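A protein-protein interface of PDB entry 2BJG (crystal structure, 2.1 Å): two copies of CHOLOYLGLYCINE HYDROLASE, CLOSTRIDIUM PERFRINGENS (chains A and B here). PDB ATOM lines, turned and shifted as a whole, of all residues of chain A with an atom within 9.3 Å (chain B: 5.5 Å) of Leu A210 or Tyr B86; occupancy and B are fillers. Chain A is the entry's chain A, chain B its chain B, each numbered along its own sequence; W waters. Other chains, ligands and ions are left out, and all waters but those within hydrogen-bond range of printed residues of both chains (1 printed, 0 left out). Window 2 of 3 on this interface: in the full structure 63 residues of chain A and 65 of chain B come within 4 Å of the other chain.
The backbone NH (N) of Val B85 lies within hydrogen-bond range of the side-chain hydroxyl (OG) of Ser B176, 3.4 Å away.
NE2 of Gln A196 lies within hydrogen-bond range of O of Gly A211 (3.0 Å).
CG of Pro B84 touches O of Leu A210, 3.7 Å away.
O of Leu A210 touches CG2 of Val B85 (3.7 Å).
Tyr B86 touches Leu A210.
Leu A210 touches Ser B176 (O to CB, 3.7 Å).
Leu A210 touches Pro B177 (CD1 to CD, 3.9 Å).
Gly A211 touches Pro B225.
Leu A210 touches just these residues of chain B: Pro B84, Val B85, Tyr B86, Ser B176 and Pro B177.
Of the printed residues of chain B, Gly A211 touches Pro B225 (3.9 Å).
Pro B84 touches just one residue of chain A: Leu A210 (3.7 Å).
Val B85 touches just one residue of chain A: Leu A210 (3.7 Å).
Tyr B86 touches one residue of chain A.
No residue of chain A comes within 4 Å of Val B87.
Ser B176 touches just one residue of chain A: Leu A210.
Printed residues of chain A within 4 Å of Pro B177: Leu A210.
Of the printed residues of chain A, Pro B225 touches Gly A211 (3.9 Å).
The nearest residue of chain B that does not touch Leu A210 is Pro B225 (4.7 Å).
The nearest residue of chain A that does not touch Tyr B86 is Thr A208 (6.4 Å).
Among the printed residues, 6 pairs touch across the chains.
No position is printed for both chains.
Water W1 lies within hydrogen-bond range of O of Leu A210 (2.7 Å) and N of Ser B176 (3.1 Å).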
ATOM      1  N   GLN A 196     -19.988 -11.870  -8.210  1.00  0.00           N
ATOM      2  CA  GLN A 196     -18.859 -12.565  -8.818  1.00  0.00           C
ATOM      3  C   GLN A 196     -17.577 -12.380  -8.009  1.00  0.00           C
ATOM      4  O   GLN A 196     -17.239 -11.269  -7.599  1.00  0.00           O
ATOM      5  CB  GLN A 196     -18.663 -12.085 -10.270  1.00  0.00           C
ATOM      6  CG  GLN A 196     -17.438 -12.656 -11.013  1.00  0.00           C
ATOM      7  CD  GLN A 196     -17.588 -14.115 -11.421  1.00  0.00           C
ATOM      8  OE1 GLN A 196     -18.446 -14.839 -10.907  1.00  0.00           O
ATOM      9  NE2 GLN A 196     -16.744 -14.558 -12.350  1.00  0.00           N
ATOM     10  N   VAL A 197     -16.895 -13.494  -7.757  1.00  0.00           N
ATOM     11  CA  VAL A 197     -15.546 -13.480  -7.195  1.00  0.00           C
ATOM     12  C   VAL A 197     -14.600 -13.734  -8.371  1.00  0.00           C
ATOM     13  O   VAL A 197     -14.515 -14.864  -8.861  1.00  0.00           O
ATOM     14  CB  VAL A 197     -15.356 -14.560  -6.098  1.00  0.00           C
ATOM     15  CG1 VAL A 197     -13.981 -14.425  -5.444  1.00  0.00           C
ATOM     16  CG2 VAL A 197     -16.463 -14.470  -5.049  1.00  0.00           C
ATOM     17  N   PRO A 198     -13.908 -12.679  -8.845  1.00  0.00           N
ATOM     18  CA  PRO A 198     -13.162 -12.783 -10.101  1.00  0.00           C
ATOM     19  C   PRO A 198     -11.804 -13.475  -9.986  1.00  0.00           C
ATOM     20  O   PRO A 198     -11.375 -14.133 -10.939  1.00  0.00           O
ATOM     21  CB  PRO A 198     -12.985 -11.319 -10.547  1.00  0.00           C
ATOM     22  CG  PRO A 198     -13.442 -10.461  -9.399  1.00  0.00           C
ATOM     23  CD  PRO A 198     -13.786 -11.342  -8.237  1.00  0.00           C
ATOM     24  N   GLU A 199     -11.143 -13.325  -8.838  1.00  0.00           N
ATOM     25  CA  GLU A 199      -9.783 -13.839  -8.653  1.00  0.00           C
ATOM     26  C   GLU A 199      -9.470 -14.255  -7.213  1.00  0.00           C
ATOM     27  O   GLU A 199     -10.160 -13.857  -6.267  1.00  0.00           O
ATOM     28  CB  GLU A 199      -8.746 -12.819  -9.147  1.00  0.00           C
ATOM     29  CG  GLU A 199      -8.549 -11.620  -8.220  1.00  0.00           C
ATOM     30  CD  GLU A 199      -7.946 -10.421  -8.931  1.00  0.00           C
ATOM     31  OE1 GLU A 199      -6.748 -10.139  -8.710  1.00  0.00           O
ATOM     32  OE2 GLU A 199      -8.669  -9.762  -9.713  1.00  0.00           O
ATOM     33  N   GLN A 205       0.479 -18.822  -7.298  1.00  0.00           N
ATOM     34  CA  GLN A 205      -0.442 -19.130  -8.387  1.00  0.00           C
ATOM     35  C   GLN A 205      -1.629 -18.160  -8.413  1.00  0.00           C
ATOM     36  O   GLN A 205      -2.331 -18.009  -7.409  1.00  0.00           O
ATOM     37  CB  GLN A 205      -0.946 -20.572  -8.248  1.00  0.00           C
ATOM     38  CG  GLN A 205      -1.936 -21.014  -9.331  1.00  0.00           C
ATOM     39  CD  GLN A 205      -1.272 -21.304 -10.670  1.00  0.00           C
ATOM     40  OE1 GLN A 205      -0.147 -21.803 -10.727  1.00  0.00           O
ATOM     41  NE2 GLN A 205      -1.977 -20.999 -11.754  1.00  0.00           N
ATOM     42  N   SER A 206      -1.847 -17.517  -9.562  1.00  0.00           N
ATOM     43  CA  SER A 206      -3.023 -16.669  -9.776  1.00  0.00           C
ATOM     44  C   SER A 206      -4.229 -17.504 -10.184  1.00  0.00           C
ATOM     45  O   SER A 206      -4.195 -18.196 -11.206  1.00  0.00           O
ATOM     46  CB  SER A 206      -2.749 -15.615 -10.852  1.00  0.00           C
ATOM     47  OG  SER A 206      -1.680 -14.770 -10.472  1.00  0.00           O
ATOM     48  N   LEU A 207      -5.287 -17.448  -9.379  1.00  0.00           N
ATOM     49  CA  LEU A 207      -6.542 -18.117  -9.722  1.00  0.00           C
ATOM     50  C   LEU A 207      -7.564 -17.103 -10.206  1.00  0.00           C
ATOM     51  O   LEU A 207      -7.858 -16.132  -9.516  1.00  0.00           O
ATOM     52  CB  LEU A 207      -7.107 -18.899  -8.536  1.00  0.00           C
ATOM     53  CG  LEU A 207      -6.264 -19.982  -7.852  1.00  0.00           C
ATOM     54  CD1 LEU A 207      -7.111 -20.662  -6.796  1.00  0.00           C
ATOM     55  CD2 LEU A 207      -5.706 -21.003  -8.852  1.00  0.00           C
ATOM     56  N   THR A 208      -8.093 -17.342 -11.400  1.00  0.00           N
ATOM     57  CA  THR A 208      -9.076 -16.458 -12.013  1.00  0.00           C
ATOM     58  C   THR A 208     -10.341 -17.233 -12.377  1.00  0.00           C
ATOM     59  O   THR A 208     -10.271 -18.344 -12.912  1.00  0.00           O
ATOM     60  CB  THR A 208      -8.502 -15.761 -13.263  1.00  0.00           C
ATOM     61  OG1 THR A 208      -7.777 -16.717 -14.047  1.00  0.00           O
ATOM     62  CG2 THR A 208      -7.551 -14.629 -12.865  1.00  0.00           C
ATOM     63  N   ALA A 209     -11.492 -16.641 -12.068  1.00  0.00           N
ATOM     64  CA  ALA A 209     -12.793 -17.241 -12.359  1.00  0.00           C
ATOM     65  C   ALA A 209     -12.940 -17.593 -13.843  1.00  0.00           C
ATOM     66  O   ALA A 209     -12.631 -16.783 -14.712  1.00  0.00           O
ATOM     67  CB  ALA A 209     -13.907 -16.309 -11.919  1.00  0.00           C
ATOM     68  N   LEU A 210     -13.401 -18.812 -14.113  1.00  0.00           N
ATOM     69  CA  LEU A 210     -13.571 -19.316 -15.477  1.00  0.00           C
ATOM     70  C   LEU A 210     -14.815 -18.737 -16.156  1.00  0.00           C
ATOM     71  O   LEU A 210     -14.859 -18.601 -17.378  1.00  0.00           O
ATOM     72  CB  LEU A 210     -13.656 -20.848 -15.462  1.00  0.00           C
ATOM     73  CG  LEU A 210     -12.482 -21.640 -14.873  1.00  0.00           C
ATOM     74  CD1 LEU A 210     -12.923 -23.036 -14.456  1.00  0.00           C
ATOM     75  CD2 LEU A 210     -11.318 -21.715 -15.848  1.00  0.00           C
ATOM     76  N   GLY A 211     -15.824 -18.428 -15.348  1.00  0.00           N
ATOM     77  CA  GLY A 211     -17.083 -17.847 -15.811  1.00  0.00           C
ATOM     78  C   GLY A 211     -17.836 -17.238 -14.646  1.00  0.00           C
ATOM     79  O   GLY A 211     -17.368 -17.281 -13.500  1.00  0.00           O
ATOM     80  N   GLN A 212     -18.999 -16.667 -14.933  1.00  0.00           N
ATOM     81  CA  GLN A 212     -19.871 -16.100 -13.904  1.00  0.00           C
ATOM     82  C   GLN A 212     -20.414 -17.168 -12.957  1.00  0.00           C
ATOM     83  O   GLN A 212     -20.600 -18.314 -13.353  1.00  0.00           O
ATOM     84  CB  GLN A 212     -21.043 -15.346 -14.548  1.00  0.00           C
ATOM     85  CG  GLN A 212     -20.647 -14.125 -15.362  1.00  0.00           C
ATOM     86  CD  GLN A 212     -19.977 -13.048 -14.529  1.00  0.00           C
ATOM     87  OE1 GLN A 212     -20.371 -12.787 -13.392  1.00  0.00           O
ATOM     88  NE2 GLN A 212     -18.962 -12.413 -15.095  1.00  0.00           N
ATOM     89  N   GLY A 213     -20.651 -16.782 -11.706  1.00  0.00           N
ATOM     90  CA  GLY A 213     -21.319 -17.645 -10.740  1.00  0.00           C
ATOM     91  C   GLY A 213     -20.475 -18.257  -9.636  1.00  0.00           C
ATOM     92  O   GLY A 213     -20.968 -19.098  -8.877  1.00  0.00           O
ATOM     93  N   THR A 214     -19.217 -17.833  -9.524  1.00  0.00           N
ATOM     94  CA  THR A 214     -18.288 -18.438  -8.559  1.00  0.00           C
ATOM     95  C   THR A 214     -18.657 -18.239  -7.085  1.00  0.00           C
ATOM     96  O   THR A 214     -18.222 -19.016  -6.229  1.00  0.00           O
ATOM     97  CB  THR A 214     -16.820 -17.988  -8.783  1.00  0.00           C
ATOM     98  OG1 THR A 214     -16.732 -16.557  -8.728  1.00  0.00           O
ATOM     99  CG2 THR A 214     -16.298 -18.493 -10.129  1.00  0.00           C
ATOM    100  N   VAL A 217     -20.793 -21.325  -5.538  1.00  0.00           N
ATOM    101  CA  VAL A 217     -20.221 -22.678  -5.505  1.00  0.00           C
ATOM    102  C   VAL A 217     -20.446 -23.287  -4.114  1.00  0.00           C
ATOM    103  O   VAL A 217     -20.141 -22.661  -3.101  1.00  0.00           O
ATOM    104  CB  VAL A 217     -18.717 -22.687  -5.918  1.00  0.00           C
ATOM    105  CG1 VAL A 217     -18.088 -24.059  -5.701  1.00  0.00           C
ATOM    106  CG2 VAL A 217     -18.560 -22.273  -7.394  1.00  0.00           C
ATOM    107  N   PHE B  83     -16.532 -18.023 -24.529  1.00  0.00           N
ATOM    108  CA  PHE B  83     -15.334 -18.821 -24.274  1.00  0.00           C
ATOM    109  C   PHE B  83     -14.177 -17.887 -23.882  1.00  0.00           C
ATOM    110  O   PHE B  83     -13.198 -17.766 -24.617  1.00  0.00           O
ATOM    111  CB  PHE B  83     -15.002 -19.638 -25.533  1.00  0.00           C
ATOM    112  CG  PHE B  83     -14.016 -20.759 -25.314  1.00  0.00           C
ATOM    113  CD1 PHE B  83     -14.224 -21.719 -24.328  1.00  0.00           C
ATOM    114  CD2 PHE B  83     -12.902 -20.879 -26.138  1.00  0.00           C
ATOM    115  CE1 PHE B  83     -13.315 -22.759 -24.141  1.00  0.00           C
ATOM    116  CE2 PHE B  83     -11.986 -21.919 -25.962  1.00  0.00           C
ATOM    117  CZ  PHE B  83     -12.195 -22.860 -24.958  1.00  0.00           C
ATOM    118  N   PRO B  84     -14.294 -17.225 -22.709  1.00  0.00           N
ATOM    119  CA  PRO B  84     -13.449 -16.083 -22.334  1.00  0.00           C
ATOM    120  C   PRO B  84     -11.980 -16.344 -21.973  1.00  0.00           C
ATOM    121  O   PRO B  84     -11.153 -15.448 -22.150  1.00  0.00           O
ATOM    122  CB  PRO B  84     -14.181 -15.490 -21.126  1.00  0.00           C
ATOM    123  CG  PRO B  84     -14.876 -16.636 -20.521  1.00  0.00           C
ATOM    124  CD  PRO B  84     -15.284 -17.529 -21.658  1.00  0.00           C
ATOM    125  N   VAL B  85     -11.640 -17.523 -21.469  1.00  0.00           N
ATOM    126  CA  VAL B  85     -10.299 -17.690 -20.889  1.00  0.00           C
ATOM    127  C   VAL B  85      -9.265 -18.329 -21.829  1.00  0.00           C
ATOM    128  O   VAL B  85      -8.168 -17.784 -22.019  1.00  0.00           O
ATOM    129  CB  VAL B  85     -10.344 -18.428 -19.515  1.00  0.00           C
ATOM    130  CG1 VAL B  85      -8.983 -18.384 -18.832  1.00  0.00           C
ATOM    131  CG2 VAL B  85     -11.410 -17.821 -18.602  1.00  0.00           C
ATOM    132  N   TYR B  86      -9.619 -19.468 -22.421  1.00  0.00           N
ATOM    133  CA  TYR B  86      -8.653 -20.303 -23.142  1.00  0.00           C
ATOM    134  C   TYR B  86      -8.688 -20.138 -24.664  1.00  0.00           C
ATOM    135  O   TYR B  86      -8.099 -20.941 -25.395  1.00  0.00           O
ATOM    136  CB  TYR B  86      -8.820 -21.774 -22.735  1.00  0.00           C
ATOM    137  CG  TYR B  86      -8.628 -22.001 -21.249  1.00  0.00           C
ATOM    138  CD1 TYR B  86      -9.709 -21.933 -20.368  1.00  0.00           C
ATOM    139  CD2 TYR B  86      -7.367 -22.272 -20.721  1.00  0.00           C
ATOM    140  CE1 TYR B  86      -9.536 -22.124 -19.001  1.00  0.00           C
ATOM    141  CE2 TYR B  86      -7.186 -22.473 -19.354  1.00  0.00           C
ATOM    142  CZ  TYR B  86      -8.275 -22.397 -18.503  1.00  0.00           C
ATOM    143  OH  TYR B  86      -8.104 -22.588 -17.151  1.00  0.00           O
ATOM    144  N   VAL B  87      -9.366 -19.092 -25.136  1.00  0.00           N
ATOM    145  CA  VAL B  87      -9.406 -18.791 -26.566  1.00  0.00           C
ATOM    146  C   VAL B  87      -8.180 -17.967 -26.979  1.00  0.00           C
ATOM    147  O   VAL B  87      -7.620 -17.216 -26.168  1.00  0.00           O
ATOM    148  CB  VAL B  87     -10.738 -18.090 -26.983  1.00  0.00           C
ATOM    149  CG1 VAL B  87     -10.712 -16.594 -26.668  1.00  0.00           C
ATOM    150  CG2 VAL B  87     -11.025 -18.317 -28.456  1.00  0.00           C
ATOM    151  N   SER B  88      -7.752 -18.138 -28.230  1.00  0.00           N
ATOM    152  CA  SER B  88      -6.687 -17.318 -28.805  1.00  0.00           C
ATOM    153  C   SER B  88      -6.842 -17.188 -30.318  1.00  0.00           C
ATOM    154  O   SER B  88      -6.495 -18.103 -31.065  1.00  0.00           O
ATOM    155  CB  SER B  88      -5.306 -17.876 -28.446  1.00  0.00           C
ATOM    156  OG  SER B  88      -4.273 -17.005 -28.882  1.00  0.00           O
ATOM    157  N   GLN B 158     -10.526 -22.698 -30.732  1.00  0.00           N
ATOM    158  CA  GLN B 158      -9.179 -22.262 -31.097  1.00  0.00           C
ATOM    159  C   GLN B 158      -8.364 -21.826 -29.880  1.00  0.00           C
ATOM    160  O   GLN B 158      -8.735 -20.899 -29.159  1.00  0.00           O
ATOM    161  CB  GLN B 158      -9.193 -21.163 -32.167  1.00  0.00           C
ATOM    162  CG  GLN B 158      -7.784 -20.794 -32.654  1.00  0.00           C
ATOM    163  CD  GLN B 158      -7.752 -20.238 -34.057  1.00  0.00           C
ATOM    164  OE1 GLN B 158      -8.232 -20.865 -35.002  1.00  0.00           O
ATOM    165  NE2 GLN B 158      -7.157 -19.059 -34.207  1.00  0.00           N
ATOM    166  N   THR B 159      -7.251 -22.518 -29.668  1.00  0.00           N
ATOM    167  CA  THR B 159      -6.309 -22.188 -28.606  1.00  0.00           C
ATOM    168  C   THR B 159      -5.040 -21.583 -29.213  1.00  0.00           C
ATOM    169  O   THR B 159      -4.926 -21.455 -30.436  1.00  0.00           O
ATOM    170  CB  THR B 159      -5.938 -23.436 -27.769  1.00  0.00           C
ATOM    171  OG1 THR B 159      -5.313 -24.414 -28.615  1.00  0.00           O
ATOM    172  CG2 THR B 159      -7.183 -24.039 -27.102  1.00  0.00           C
ATOM    173  N   LYS B 160      -4.095 -21.214 -28.350  1.00  0.00           N
ATOM    174  CA  LYS B 160      -2.818 -20.639 -28.782  1.00  0.00           C
ATOM    175  C   LYS B 160      -2.037 -21.557 -29.727  1.00  0.00           C
ATOM    176  O   LYS B 160      -1.307 -21.078 -30.596  1.00  0.00           O
ATOM    177  CB  LYS B 160      -1.956 -20.249 -27.572  1.00  0.00           C
ATOM    178  CG  LYS B 160      -1.688 -21.381 -26.579  1.00  0.00           C
ATOM    179  CD  LYS B 160      -0.644 -20.975 -25.557  1.00  0.00           C
ATOM    180  CE  LYS B 160      -0.184 -22.170 -24.740  1.00  0.00           C
ATOM    181  NZ  LYS B 160       0.970 -21.808 -23.872  1.00  0.00           N
ATOM    182  N   SER B 176     -16.061 -21.889 -20.643  1.00  0.00           N
ATOM    183  CA  SER B 176     -14.695 -22.252 -20.220  1.00  0.00           C
ATOM    184  C   SER B 176     -14.682 -23.141 -18.969  1.00  0.00           C
ATOM    185  O   SER B 176     -15.561 -23.004 -18.114  1.00  0.00           O
ATOM    186  CB  SER B 176     -13.847 -20.990 -19.987  1.00  0.00           C
ATOM    187  OG  SER B 176     -13.662 -20.282 -21.206  1.00  0.00           O
ATOM    188  N   PRO B 177     -13.681 -24.042 -18.841  1.00  0.00           N
ATOM    189  CA  PRO B 177     -12.494 -24.261 -19.688  1.00  0.00           C
ATOM    190  C   PRO B 177     -12.740 -25.100 -20.948  1.00  0.00           C
ATOM    191  O   PRO B 177     -13.886 -25.253 -21.365  1.00  0.00           O
ATOM    192  CB  PRO B 177     -11.507 -24.971 -18.747  1.00  0.00           C
ATOM    193  CG  PRO B 177     -12.277 -25.369 -17.537  1.00  0.00           C
ATOM    194  CD  PRO B 177     -13.709 -24.978 -17.702  1.00  0.00           C
ATOM    195  N   THR B 178     -11.659 -25.622 -21.543  1.00  0.00           N
ATOM    196  CA  THR B 178     -11.709 -26.357 -22.814  1.00  0.00           C
ATOM    197  C   THR B 178     -12.578 -27.604 -22.728  1.00  0.00           C
ATOM    198  O   THR B 178     -12.821 -28.109 -21.634  1.00  0.00           O
ATOM    199  CB  THR B 178     -10.297 -26.775 -23.304  1.00  0.00           C
ATOM    200  OG1 THR B 178      -9.683 -27.628 -22.331  1.00  0.00           O
ATOM    201  CG2 THR B 178      -9.413 -25.551 -23.543  1.00  0.00           C
ATOM    202  N   PRO B 225     -19.954 -22.412 -15.538  1.00  0.00           N
ATOM    203  CA  PRO B 225     -19.941 -23.275 -16.726  1.00  0.00           C
ATOM    204  C   PRO B 225     -19.713 -24.764 -16.416  1.00  0.00           C
ATOM    205  O   PRO B 225     -20.392 -25.617 -16.995  1.00  0.00           O
ATOM    206  CB  PRO B 225     -18.785 -22.706 -17.558  1.00  0.00           C
ATOM    207  CG  PRO B 225     -18.673 -21.283 -17.132  1.00  0.00           C
ATOM    208  CD  PRO B 225     -19.002 -21.287 -15.669  1.00  0.00           C
HETATM  209  O   HOH W   1     -16.701 -19.205 -19.284  1.00  0.00           O
